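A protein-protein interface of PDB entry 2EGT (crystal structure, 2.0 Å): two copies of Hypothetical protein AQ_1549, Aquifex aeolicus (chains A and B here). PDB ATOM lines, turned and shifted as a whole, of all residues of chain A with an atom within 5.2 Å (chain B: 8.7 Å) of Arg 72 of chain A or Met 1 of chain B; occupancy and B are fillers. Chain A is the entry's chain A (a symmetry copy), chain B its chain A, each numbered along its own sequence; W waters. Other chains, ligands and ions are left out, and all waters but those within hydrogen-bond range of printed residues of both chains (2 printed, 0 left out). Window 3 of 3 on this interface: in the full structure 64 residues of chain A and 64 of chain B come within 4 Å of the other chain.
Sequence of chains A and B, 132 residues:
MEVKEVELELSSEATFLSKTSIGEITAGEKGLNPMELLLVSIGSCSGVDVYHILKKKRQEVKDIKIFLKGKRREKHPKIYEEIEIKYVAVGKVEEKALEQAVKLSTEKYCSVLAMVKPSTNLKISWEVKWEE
O of Lys 4 of chain B is in hydrogen-bond range of N of Gly 70 of chain A, at 2.7 Å.
The guanidinium group of Arg 72 of chain A is in hydrogen-bond range of the side-chain hydroxyl of Ser 111 of chain B (3.0 Å).
The side-chain sulfur (SD) of Met 115 of chain B sits at hydrogen-bond distance from the backbone NH (N) of Tyr 80 of chain A (3.6 Å).
The side-chain hydroxyl (OG) of Ser 111 of chain B lies within hydrogen-bond range of the backbone carbonyl oxygen (O) of Lys 78 of chain A, 3.0 Å away.
The guanidinium group (NH1) of Arg 72 of chain A is in salt-bridge range of the side-chain carboxylate (OE2) of Glu 2 of chain B, 2.8 Å away.
O of Lys 71 of chain A sits at hydrogen-bond distance from N of Glu 81 of chain A, at 2.8 Å.
The backbone NH (N) of Val 112 of chain B sits at hydrogen-bond distance from the side-chain sulfur (SG) of Cys 45 of chain B (3.4 Å).
SG of Cys 45 of chain B is in hydrogen-bond range of N of Ser 111 of chain B.
The guanidinium group (NE) of Arg 72 of chain A is in hydrogen-bond range of the backbone carbonyl oxygen (O) of Lys 78 of chain A (2.8 Å).
The backbone NH (N) of Val 112 of chain B lies close to the side-chain sulfur (SG) of Cys 110 of chain B, 3.6 Å away.
SG of Cys 110 of chain B forms a disulfide with SG of Cys 45 of chain B (2.1 Å).
Among the printed residues, merely in contact across the chains: Met 35 of chain A with Ser 111 of chain B, Met 35 of chain A with Val 112 of chain B, Gly 70 of chain A with Glu 2 of chain B, Gly 70 of chain A with Val 3 of chain B, Lys 71 of chain A with Glu 2 of chain B, Arg 72 of chain A with Met 1 of chain B, Arg 72 of chain A with Lys 4 of chain B, Ile 79 of chain A with Ser 111 of chain B, Ile 79 of chain A with Met 115 of chain B and Tyr 80 of chain A with Lys 4 of chain B.
Printed residues of chain B within 4 Å of Arg 72 of chain A: Met 1, Glu 2, Lys 4 and Ser 111.
Of chain A, only Arg 72 (3.1 Å) comes within 4 Å of Met 1 of chain B.
Of the printed residues of chain B, Met 35 of chain A touches Ser 111 (3.8 Å) and Val 112 (3.6 Å).
Of the printed residues of chain A, Met 115 of chain B touches Ile 79 and Tyr 80.
Of the printed residues of chain B, Lys 71 of chain A touches Glu 2.
Printed residues of chain A within 4 Å of Val 112 of chain B: Met 35 (3.6 Å).
Of the printed residues of chain B, Gly 70 of chain A touches Glu 2 (3.8 Å), Val 3 (3.3 Å) and Lys 4 (2.7 Å).
Arg 73 of chain A touches none of the printed residues of chain B.
Cys 110 of chain B touches none of the printed residues of chain A.
The nearest residue of chain A that does not touch Met 1 of chain B is Lys 71 of chain A (4.1 Å).
The nearest printed residue of chain B that does not touch Met 35 of chain A is Met 115 of chain B (4.3 Å).
Of the 10 printed residues of chain A, 7 touch a printed residue of chain B.
Hydrophobic or aromatic side chains of chain A that line the printed part of chain B: Met 35, Ile 79 and Tyr 80.
Of the 12 printed residues of chain B, 7 touch a printed residue of chain A.
Printed residues of chain B that touch a printed residue of chain A: Met 1, Glu 2, Val 3, Lys 4, Ser 111, Val 112 and Met 115.
Hydrophobic or aromatic side chains of chain B within 4 Å of the printed part of chain A: Met 1, Val 3, Val 112 and Met 115.
No position is printed for both chains.
Water W1 lies within hydrogen-bond range of NZ of Lys 71 of chain A and O of Met 1 of chain B.
Water W2 lies within hydrogen-bond range of the backbone carbonyl oxygen of Tyr 109 of chain B (2.7 Å), the backbone NH of Lys 78 of chain A (2.8 Å) and the side-chain hydroxyl of Ser 111 of chain B (3.0 Å).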
ATOM      1  N   MET A  35     -11.206  14.632 -30.035  1.00  0.00           N
ATOM      2  CA  MET A  35     -10.882  13.716 -28.946  1.00  0.00           C
ATOM      3  C   MET A  35     -11.848  12.534 -28.885  1.00  0.00           C
ATOM      4  O   MET A  35     -11.481  11.447 -28.424  1.00  0.00           O
ATOM      5  CB  MET A  35     -10.827  14.464 -27.606  1.00  0.00           C
ATOM      6  CG  MET A  35      -9.498  15.219 -27.395  1.00  0.00           C
ATOM      7  SD  MET A  35      -8.076  14.128 -27.062  1.00  0.00           S
ATOM      8  CE  MET A  35      -8.117  14.114 -25.232  1.00  0.00           C
ATOM      9  N   GLY A  70     -13.264   8.674 -21.520  1.00  0.00           N
ATOM     10  CA  GLY A  70     -12.001   9.348 -21.295  1.00  0.00           C
ATOM     11  C   GLY A  70     -12.152  10.542 -20.372  1.00  0.00           C
ATOM     12  O   GLY A  70     -12.997  11.407 -20.591  1.00  0.00           O
ATOM     13  N   LYS A  71     -11.318  10.581 -19.340  1.00  0.00           N
ATOM     14  CA  LYS A  71     -11.323  11.655 -18.351  1.00  0.00           C
ATOM     15  C   LYS A  71     -10.163  12.582 -18.718  1.00  0.00           C
ATOM     16  O   LYS A  71      -9.004  12.184 -18.639  1.00  0.00           O
ATOM     17  CB  LYS A  71     -11.107  11.041 -16.961  1.00  0.00           C
ATOM     18  CG  LYS A  71     -11.439  11.918 -15.764  1.00  0.00           C
ATOM     19  CD  LYS A  71     -11.110  11.151 -14.479  1.00  0.00           C
ATOM     20  CE  LYS A  71     -11.420  11.944 -13.216  1.00  0.00           C
ATOM     21  NZ  LYS A  71     -12.882  12.123 -13.004  1.00  0.00           N
ATOM     22  N   ARG A  72     -10.478  13.805 -19.126  1.00  0.00           N
ATOM     23  CA  ARG A  72      -9.457  14.765 -19.530  1.00  0.00           C
ATOM     24  C   ARG A  72      -8.912  15.588 -18.374  1.00  0.00           C
ATOM     25  O   ARG A  72      -9.649  15.962 -17.458  1.00  0.00           O
ATOM     26  CB  ARG A  72     -10.015  15.727 -20.581  1.00  0.00           C
ATOM     27  CG  ARG A  72     -10.564  15.058 -21.826  1.00  0.00           C
ATOM     28  CD  ARG A  72     -11.027  16.090 -22.844  1.00  0.00           C
ATOM     29  NE  ARG A  72      -9.916  16.809 -23.463  1.00  0.00           N
ATOM     30  CZ  ARG A  72     -10.062  17.707 -24.434  1.00  0.00           C
ATOM     31  NH1 ARG A  72     -11.275  18.000 -24.890  1.00  0.00           N
ATOM     32  NH2 ARG A  72      -8.999  18.297 -24.970  1.00  0.00           N
ATOM     33  N   ARG A  73      -7.619  15.887 -18.421  1.00  0.00           N
ATOM     34  CA  ARG A  73      -7.033  16.685 -17.362  1.00  0.00           C
ATOM     35  C   ARG A  73      -7.448  18.140 -17.559  1.00  0.00           C
ATOM     36  O   ARG A  73      -7.908  18.532 -18.635  1.00  0.00           O
ATOM     37  CB  ARG A  73      -5.508  16.538 -17.338  1.00  0.00           C
ATOM     38  CG  ARG A  73      -4.751  17.279 -18.412  1.00  0.00           C
ATOM     39  CD  ARG A  73      -3.265  17.235 -18.085  1.00  0.00           C
ATOM     40  NE  ARG A  73      -2.520  18.276 -18.778  1.00  0.00           N
ATOM     41  CZ  ARG A  73      -1.319  18.701 -18.405  1.00  0.00           C
ATOM     42  NH1 ARG A  73      -0.725  18.172 -17.344  1.00  0.00           N
ATOM     43  NH2 ARG A  73      -0.716  19.665 -19.087  1.00  0.00           N
ATOM     44  N   GLU A  74      -7.276  18.936 -16.512  1.00  0.00           N
ATOM     45  CA  GLU A  74      -7.674  20.337 -16.515  1.00  0.00           C
ATOM     46  C   GLU A  74      -6.731  21.326 -17.204  1.00  0.00           C
ATOM     47  O   GLU A  74      -7.167  22.392 -17.637  1.00  0.00           O
ATOM     48  CB  GLU A  74      -7.902  20.769 -15.065  1.00  0.00           C
ATOM     49  CG  GLU A  74      -8.596  19.691 -14.235  1.00  0.00           C
ATOM     50  CD  GLU A  74      -8.499  19.930 -12.741  1.00  0.00           C
ATOM     51  OE1 GLU A  74      -7.367  20.103 -12.236  1.00  0.00           O
ATOM     52  OE2 GLU A  74      -9.555  19.932 -12.071  1.00  0.00           O
ATOM     53  N   LYS A  78      -4.847  19.219 -22.706  1.00  0.00           N
ATOM     54  CA  LYS A  78      -5.893  18.489 -22.006  1.00  0.00           C
ATOM     55  C   LYS A  78      -6.081  17.055 -22.488  1.00  0.00           C
ATOM     56  O   LYS A  78      -7.137  16.683 -23.002  1.00  0.00           O
ATOM     57  CB  LYS A  78      -7.204  19.276 -22.098  1.00  0.00           C
ATOM     58  CG  LYS A  78      -7.073  20.670 -21.496  1.00  0.00           C
ATOM     59  CD  LYS A  78      -8.357  21.474 -21.547  1.00  0.00           C
ATOM     60  CE  LYS A  78      -8.154  22.813 -20.841  1.00  0.00           C
ATOM     61  NZ  LYS A  78      -9.383  23.648 -20.786  1.00  0.00           N
ATOM     62  N   ILE A  79      -5.042  16.253 -22.290  1.00  0.00           N
ATOM     63  CA  ILE A  79      -5.042  14.846 -22.670  1.00  0.00           C
ATOM     64  C   ILE A  79      -5.946  14.053 -21.734  1.00  0.00           C
ATOM     65  O   ILE A  79      -6.434  14.573 -20.729  1.00  0.00           O
ATOM     66  CB  ILE A  79      -3.633  14.239 -22.546  1.00  0.00           C
ATOM     67  CG1 ILE A  79      -3.196  14.263 -21.077  1.00  0.00           C
ATOM     68  CG2 ILE A  79      -2.640  15.033 -23.394  1.00  0.00           C
ATOM     69  CD1 ILE A  79      -1.955  13.449 -20.780  1.00  0.00           C
ATOM     70  N   TYR A  80      -6.166  12.787 -22.070  1.00  0.00           N
ATOM     71  CA  TYR A  80      -6.970  11.916 -21.228  1.00  0.00           C
ATOM     72  C   TYR A  80      -6.030  11.410 -20.135  1.00  0.00           C
ATOM     73  O   TYR A  80      -5.049  10.736 -20.439  1.00  0.00           O
ATOM     74  CB  TYR A  80      -7.492  10.713 -22.025  1.00  0.00           C
ATOM     75  CG  TYR A  80      -8.593  11.018 -23.021  1.00  0.00           C
ATOM     76  CD1 TYR A  80      -9.777  11.644 -22.618  1.00  0.00           C
ATOM     77  CD2 TYR A  80      -8.474  10.636 -24.359  1.00  0.00           C
ATOM     78  CE1 TYR A  80     -10.814  11.877 -23.525  1.00  0.00           C
ATOM     79  CE2 TYR A  80      -9.506  10.864 -25.273  1.00  0.00           C
ATOM     80  CZ  TYR A  80     -10.669  11.482 -24.853  1.00  0.00           C
ATOM     81  OH  TYR A  80     -11.683  11.711 -25.755  1.00  0.00           O
ATOM     82  N   GLU A  81      -6.300  11.741 -18.875  1.00  0.00           N
ATOM     83  CA  GLU A  81      -5.443  11.249 -17.797  1.00  0.00           C
ATOM     84  C   GLU A  81      -5.702   9.760 -17.666  1.00  0.00           C
ATOM     85  O   GLU A  81      -4.864   9.004 -17.175  1.00  0.00           O
ATOM     86  CB  GLU A  81      -5.761  11.931 -16.466  1.00  0.00           C
ATOM     87  CG  GLU A  81      -5.388  13.392 -16.408  1.00  0.00           C
ATOM     88  CD  GLU A  81      -5.460  13.943 -14.998  1.00  0.00           C
ATOM     89  OE1 GLU A  81      -6.517  13.786 -14.349  1.00  0.00           O
ATOM     90  OE2 GLU A  81      -4.459  14.533 -14.541  1.00  0.00           O
ATOM     91  N   MET B   1     -12.656  18.185 -14.775  1.00  0.00           N
ATOM     92  CA  MET B   1     -12.181  17.165 -15.756  1.00  0.00           C
ATOM     93  C   MET B   1     -13.336  16.685 -16.626  1.00  0.00           C
ATOM     94  O   MET B   1     -14.096  15.796 -16.232  1.00  0.00           O
ATOM     95  CB  MET B   1     -11.557  15.982 -15.023  1.00  0.00           C
ATOM     96  N   GLU B   2     -13.462  17.280 -17.810  1.00  0.00           N
ATOM     97  CA  GLU B   2     -14.523  16.917 -18.737  1.00  0.00           C
ATOM     98  C   GLU B   2     -14.388  15.448 -19.130  1.00  0.00           C
ATOM     99  O   GLU B   2     -13.284  14.904 -19.184  1.00  0.00           O
ATOM    100  CB  GLU B   2     -14.470  17.806 -19.983  1.00  0.00           C
ATOM    101  CG  GLU B   2     -13.268  17.571 -20.873  1.00  0.00           C
ATOM    102  CD  GLU B   2     -13.143  18.613 -21.970  1.00  0.00           C
ATOM    103  OE1 GLU B   2     -12.749  19.761 -21.664  1.00  0.00           O
ATOM    104  OE2 GLU B   2     -13.445  18.288 -23.138  1.00  0.00           O
ATOM    105  N   VAL B   3     -15.520  14.811 -19.399  1.00  0.00           N
ATOM    106  CA  VAL B   3     -15.527  13.406 -19.768  1.00  0.00           C
ATOM    107  C   VAL B   3     -16.065  13.183 -21.176  1.00  0.00           C
ATOM    108  O   VAL B   3     -17.087  13.751 -21.554  1.00  0.00           O
ATOM    109  CB  VAL B   3     -16.379  12.588 -18.773  1.00  0.00           C
ATOM    110  CG1 VAL B   3     -16.413  11.125 -19.188  1.00  0.00           C
ATOM    111  CG2 VAL B   3     -15.808  12.727 -17.367  1.00  0.00           C
ATOM    112  N   LYS B   4     -15.362  12.357 -21.947  1.00  0.00           N
ATOM    113  CA  LYS B   4     -15.775  12.025 -23.306  1.00  0.00           C
ATOM    114  C   LYS B   4     -16.165  10.546 -23.320  1.00  0.00           C
ATOM    115  O   LYS B   4     -15.434   9.703 -22.797  1.00  0.00           O
ATOM    116  CB  LYS B   4     -14.625  12.251 -24.295  1.00  0.00           C
ATOM    117  CG  LYS B   4     -14.127  13.687 -24.404  1.00  0.00           C
ATOM    118  CD  LYS B   4     -15.149  14.597 -25.063  1.00  0.00           C
ATOM    119  CE  LYS B   4     -14.581  15.999 -25.264  1.00  0.00           C
ATOM    120  NZ  LYS B   4     -15.562  16.916 -25.916  1.00  0.00           N
ATOM    121  N   GLU B   5     -17.311  10.234 -23.916  1.00  0.00           N
ATOM    122  CA  GLU B   5     -17.782   8.854 -23.989  1.00  0.00           C
ATOM    123  C   GLU B   5     -18.248   8.472 -25.388  1.00  0.00           C
ATOM    124  O   GLU B   5     -18.983   9.215 -26.035  1.00  0.00           O
ATOM    125  CB  GLU B   5     -18.946   8.627 -23.024  1.00  0.00           C
ATOM    126  CG  GLU B   5     -18.635   8.883 -21.567  1.00  0.00           C
ATOM    127  CD  GLU B   5     -19.797   8.505 -20.666  1.00  0.00           C
ATOM    128  OE1 GLU B   5     -20.182   7.316 -20.661  1.00  0.00           O
ATOM    129  OE2 GLU B   5     -20.324   9.394 -19.966  1.00  0.00           O
ATOM    130  N   CYS B  45      -7.617  18.091 -34.543  1.00  0.00           N
ATOM    131  CA  CYS B  45      -7.288  18.599 -33.213  1.00  0.00           C
ATOM    132  C   CYS B  45      -6.367  19.791 -33.389  1.00  0.00           C
ATOM    133  O   CYS B  45      -6.642  20.893 -32.909  1.00  0.00           O
ATOM    134  CB  CYS B  45      -6.549  17.512 -32.444  1.00  0.00           C
ATOM    135  SG  CYS B  45      -5.778  17.831 -30.812  1.00  0.00           S
ATOM    136  N   ASP B  49      -6.744  24.243 -33.387  1.00  0.00           N
ATOM    137  CA  ASP B  49      -5.873  25.156 -32.640  1.00  0.00           C
ATOM    138  C   ASP B  49      -5.327  26.216 -33.580  1.00  0.00           C
ATOM    139  O   ASP B  49      -5.362  27.407 -33.279  1.00  0.00           O
ATOM    140  CB  ASP B  49      -4.659  24.438 -32.037  1.00  0.00           C
ATOM    141  CG  ASP B  49      -5.025  23.390 -31.005  1.00  0.00           C
ATOM    142  OD1 ASP B  49      -6.033  23.553 -30.290  1.00  0.00           O
ATOM    143  OD2 ASP B  49      -4.268  22.403 -30.897  1.00  0.00           O
ATOM    144  N   TYR B 109      -1.167  23.026 -27.082  1.00  0.00           N
ATOM    145  CA  TYR B 109      -2.610  22.840 -27.179  1.00  0.00           C
ATOM    146  C   TYR B 109      -3.256  21.553 -27.676  1.00  0.00           C
ATOM    147  O   TYR B 109      -4.134  21.023 -26.996  1.00  0.00           O
ATOM    148  CB  TYR B 109      -3.209  24.018 -27.947  1.00  0.00           C
ATOM    149  CG  TYR B 109      -3.029  25.333 -27.230  1.00  0.00           C
ATOM    150  CD1 TYR B 109      -3.530  25.516 -25.942  1.00  0.00           C
ATOM    151  CD2 TYR B 109      -2.350  26.392 -27.831  1.00  0.00           C
ATOM    152  CE1 TYR B 109      -3.362  26.720 -25.270  1.00  0.00           C
ATOM    153  CE2 TYR B 109      -2.176  27.604 -27.167  1.00  0.00           C
ATOM    154  CZ  TYR B 109      -2.685  27.760 -25.886  1.00  0.00           C
ATOM    155  OH  TYR B 109      -2.522  28.953 -25.222  1.00  0.00           O
ATOM    156  N   CYS B 110      -2.863  21.037 -28.836  1.00  0.00           N
ATOM    157  CA  CYS B 110      -3.538  19.834 -29.311  1.00  0.00           C
ATOM    158  C   CYS B 110      -3.313  18.614 -28.412  1.00  0.00           C
ATOM    159  O   CYS B 110      -2.205  18.089 -28.290  1.00  0.00           O
ATOM    160  CB  CYS B 110      -3.188  19.518 -30.783  1.00  0.00           C
ATOM    161  SG  CYS B 110      -3.749  17.833 -31.168  1.00  0.00           S
ATOM    162  N   SER B 111      -4.398  18.180 -27.773  1.00  0.00           N
ATOM    163  CA  SER B 111      -4.373  17.048 -26.849  1.00  0.00           C
ATOM    164  C   SER B 111      -4.058  15.697 -27.487  1.00  0.00           C
ATOM    165  O   SER B 111      -3.348  14.879 -26.903  1.00  0.00           O
ATOM    166  CB  SER B 111      -5.716  16.945 -26.115  1.00  0.00           C
ATOM    167  OG  SER B 111      -6.011  18.136 -25.408  1.00  0.00           O
ATOM    168  N   VAL B 112      -4.597  15.449 -28.673  1.00  0.00           N
ATOM    169  CA  VAL B 112      -4.358  14.174 -29.339  1.00  0.00           C
ATOM    170  C   VAL B 112      -2.875  14.002 -29.644  1.00  0.00           C
ATOM    171  O   VAL B 112      -2.286  12.958 -29.358  1.00  0.00           O
ATOM    172  CB  VAL B 112      -5.173  14.068 -30.652  1.00  0.00           C
ATOM    173  CG1 VAL B 112      -4.922  12.714 -31.319  1.00  0.00           C
ATOM    174  CG2 VAL B 112      -6.659  14.245 -30.354  1.00  0.00           C
ATOM    175  N   MET B 115      -0.711  13.153 -26.679  1.00  0.00           N
ATOM    176  CA  MET B 115      -0.791  11.766 -26.238  1.00  0.00           C
ATOM    177  C   MET B 115       0.071  10.794 -27.045  1.00  0.00           C
ATOM    178  O   MET B 115       0.528   9.778 -26.515  1.00  0.00           O
ATOM    179  CB  MET B 115      -2.253  11.289 -26.249  1.00  0.00           C
ATOM    180  CG  MET B 115      -3.137  11.971 -25.201  1.00  0.00           C
ATOM    181  SD  MET B 115      -4.830  11.320 -25.107  1.00  0.00           S
ATOM    182  CE  MET B 115      -4.537   9.818 -24.272  1.00  0.00           C
HETATM  183  O   HOH W   1     -14.962  13.343 -14.095  1.00  0.00           O
HETATM  184  O   HOH W   2      -5.508  21.062 -24.716  1.00  0.00           O
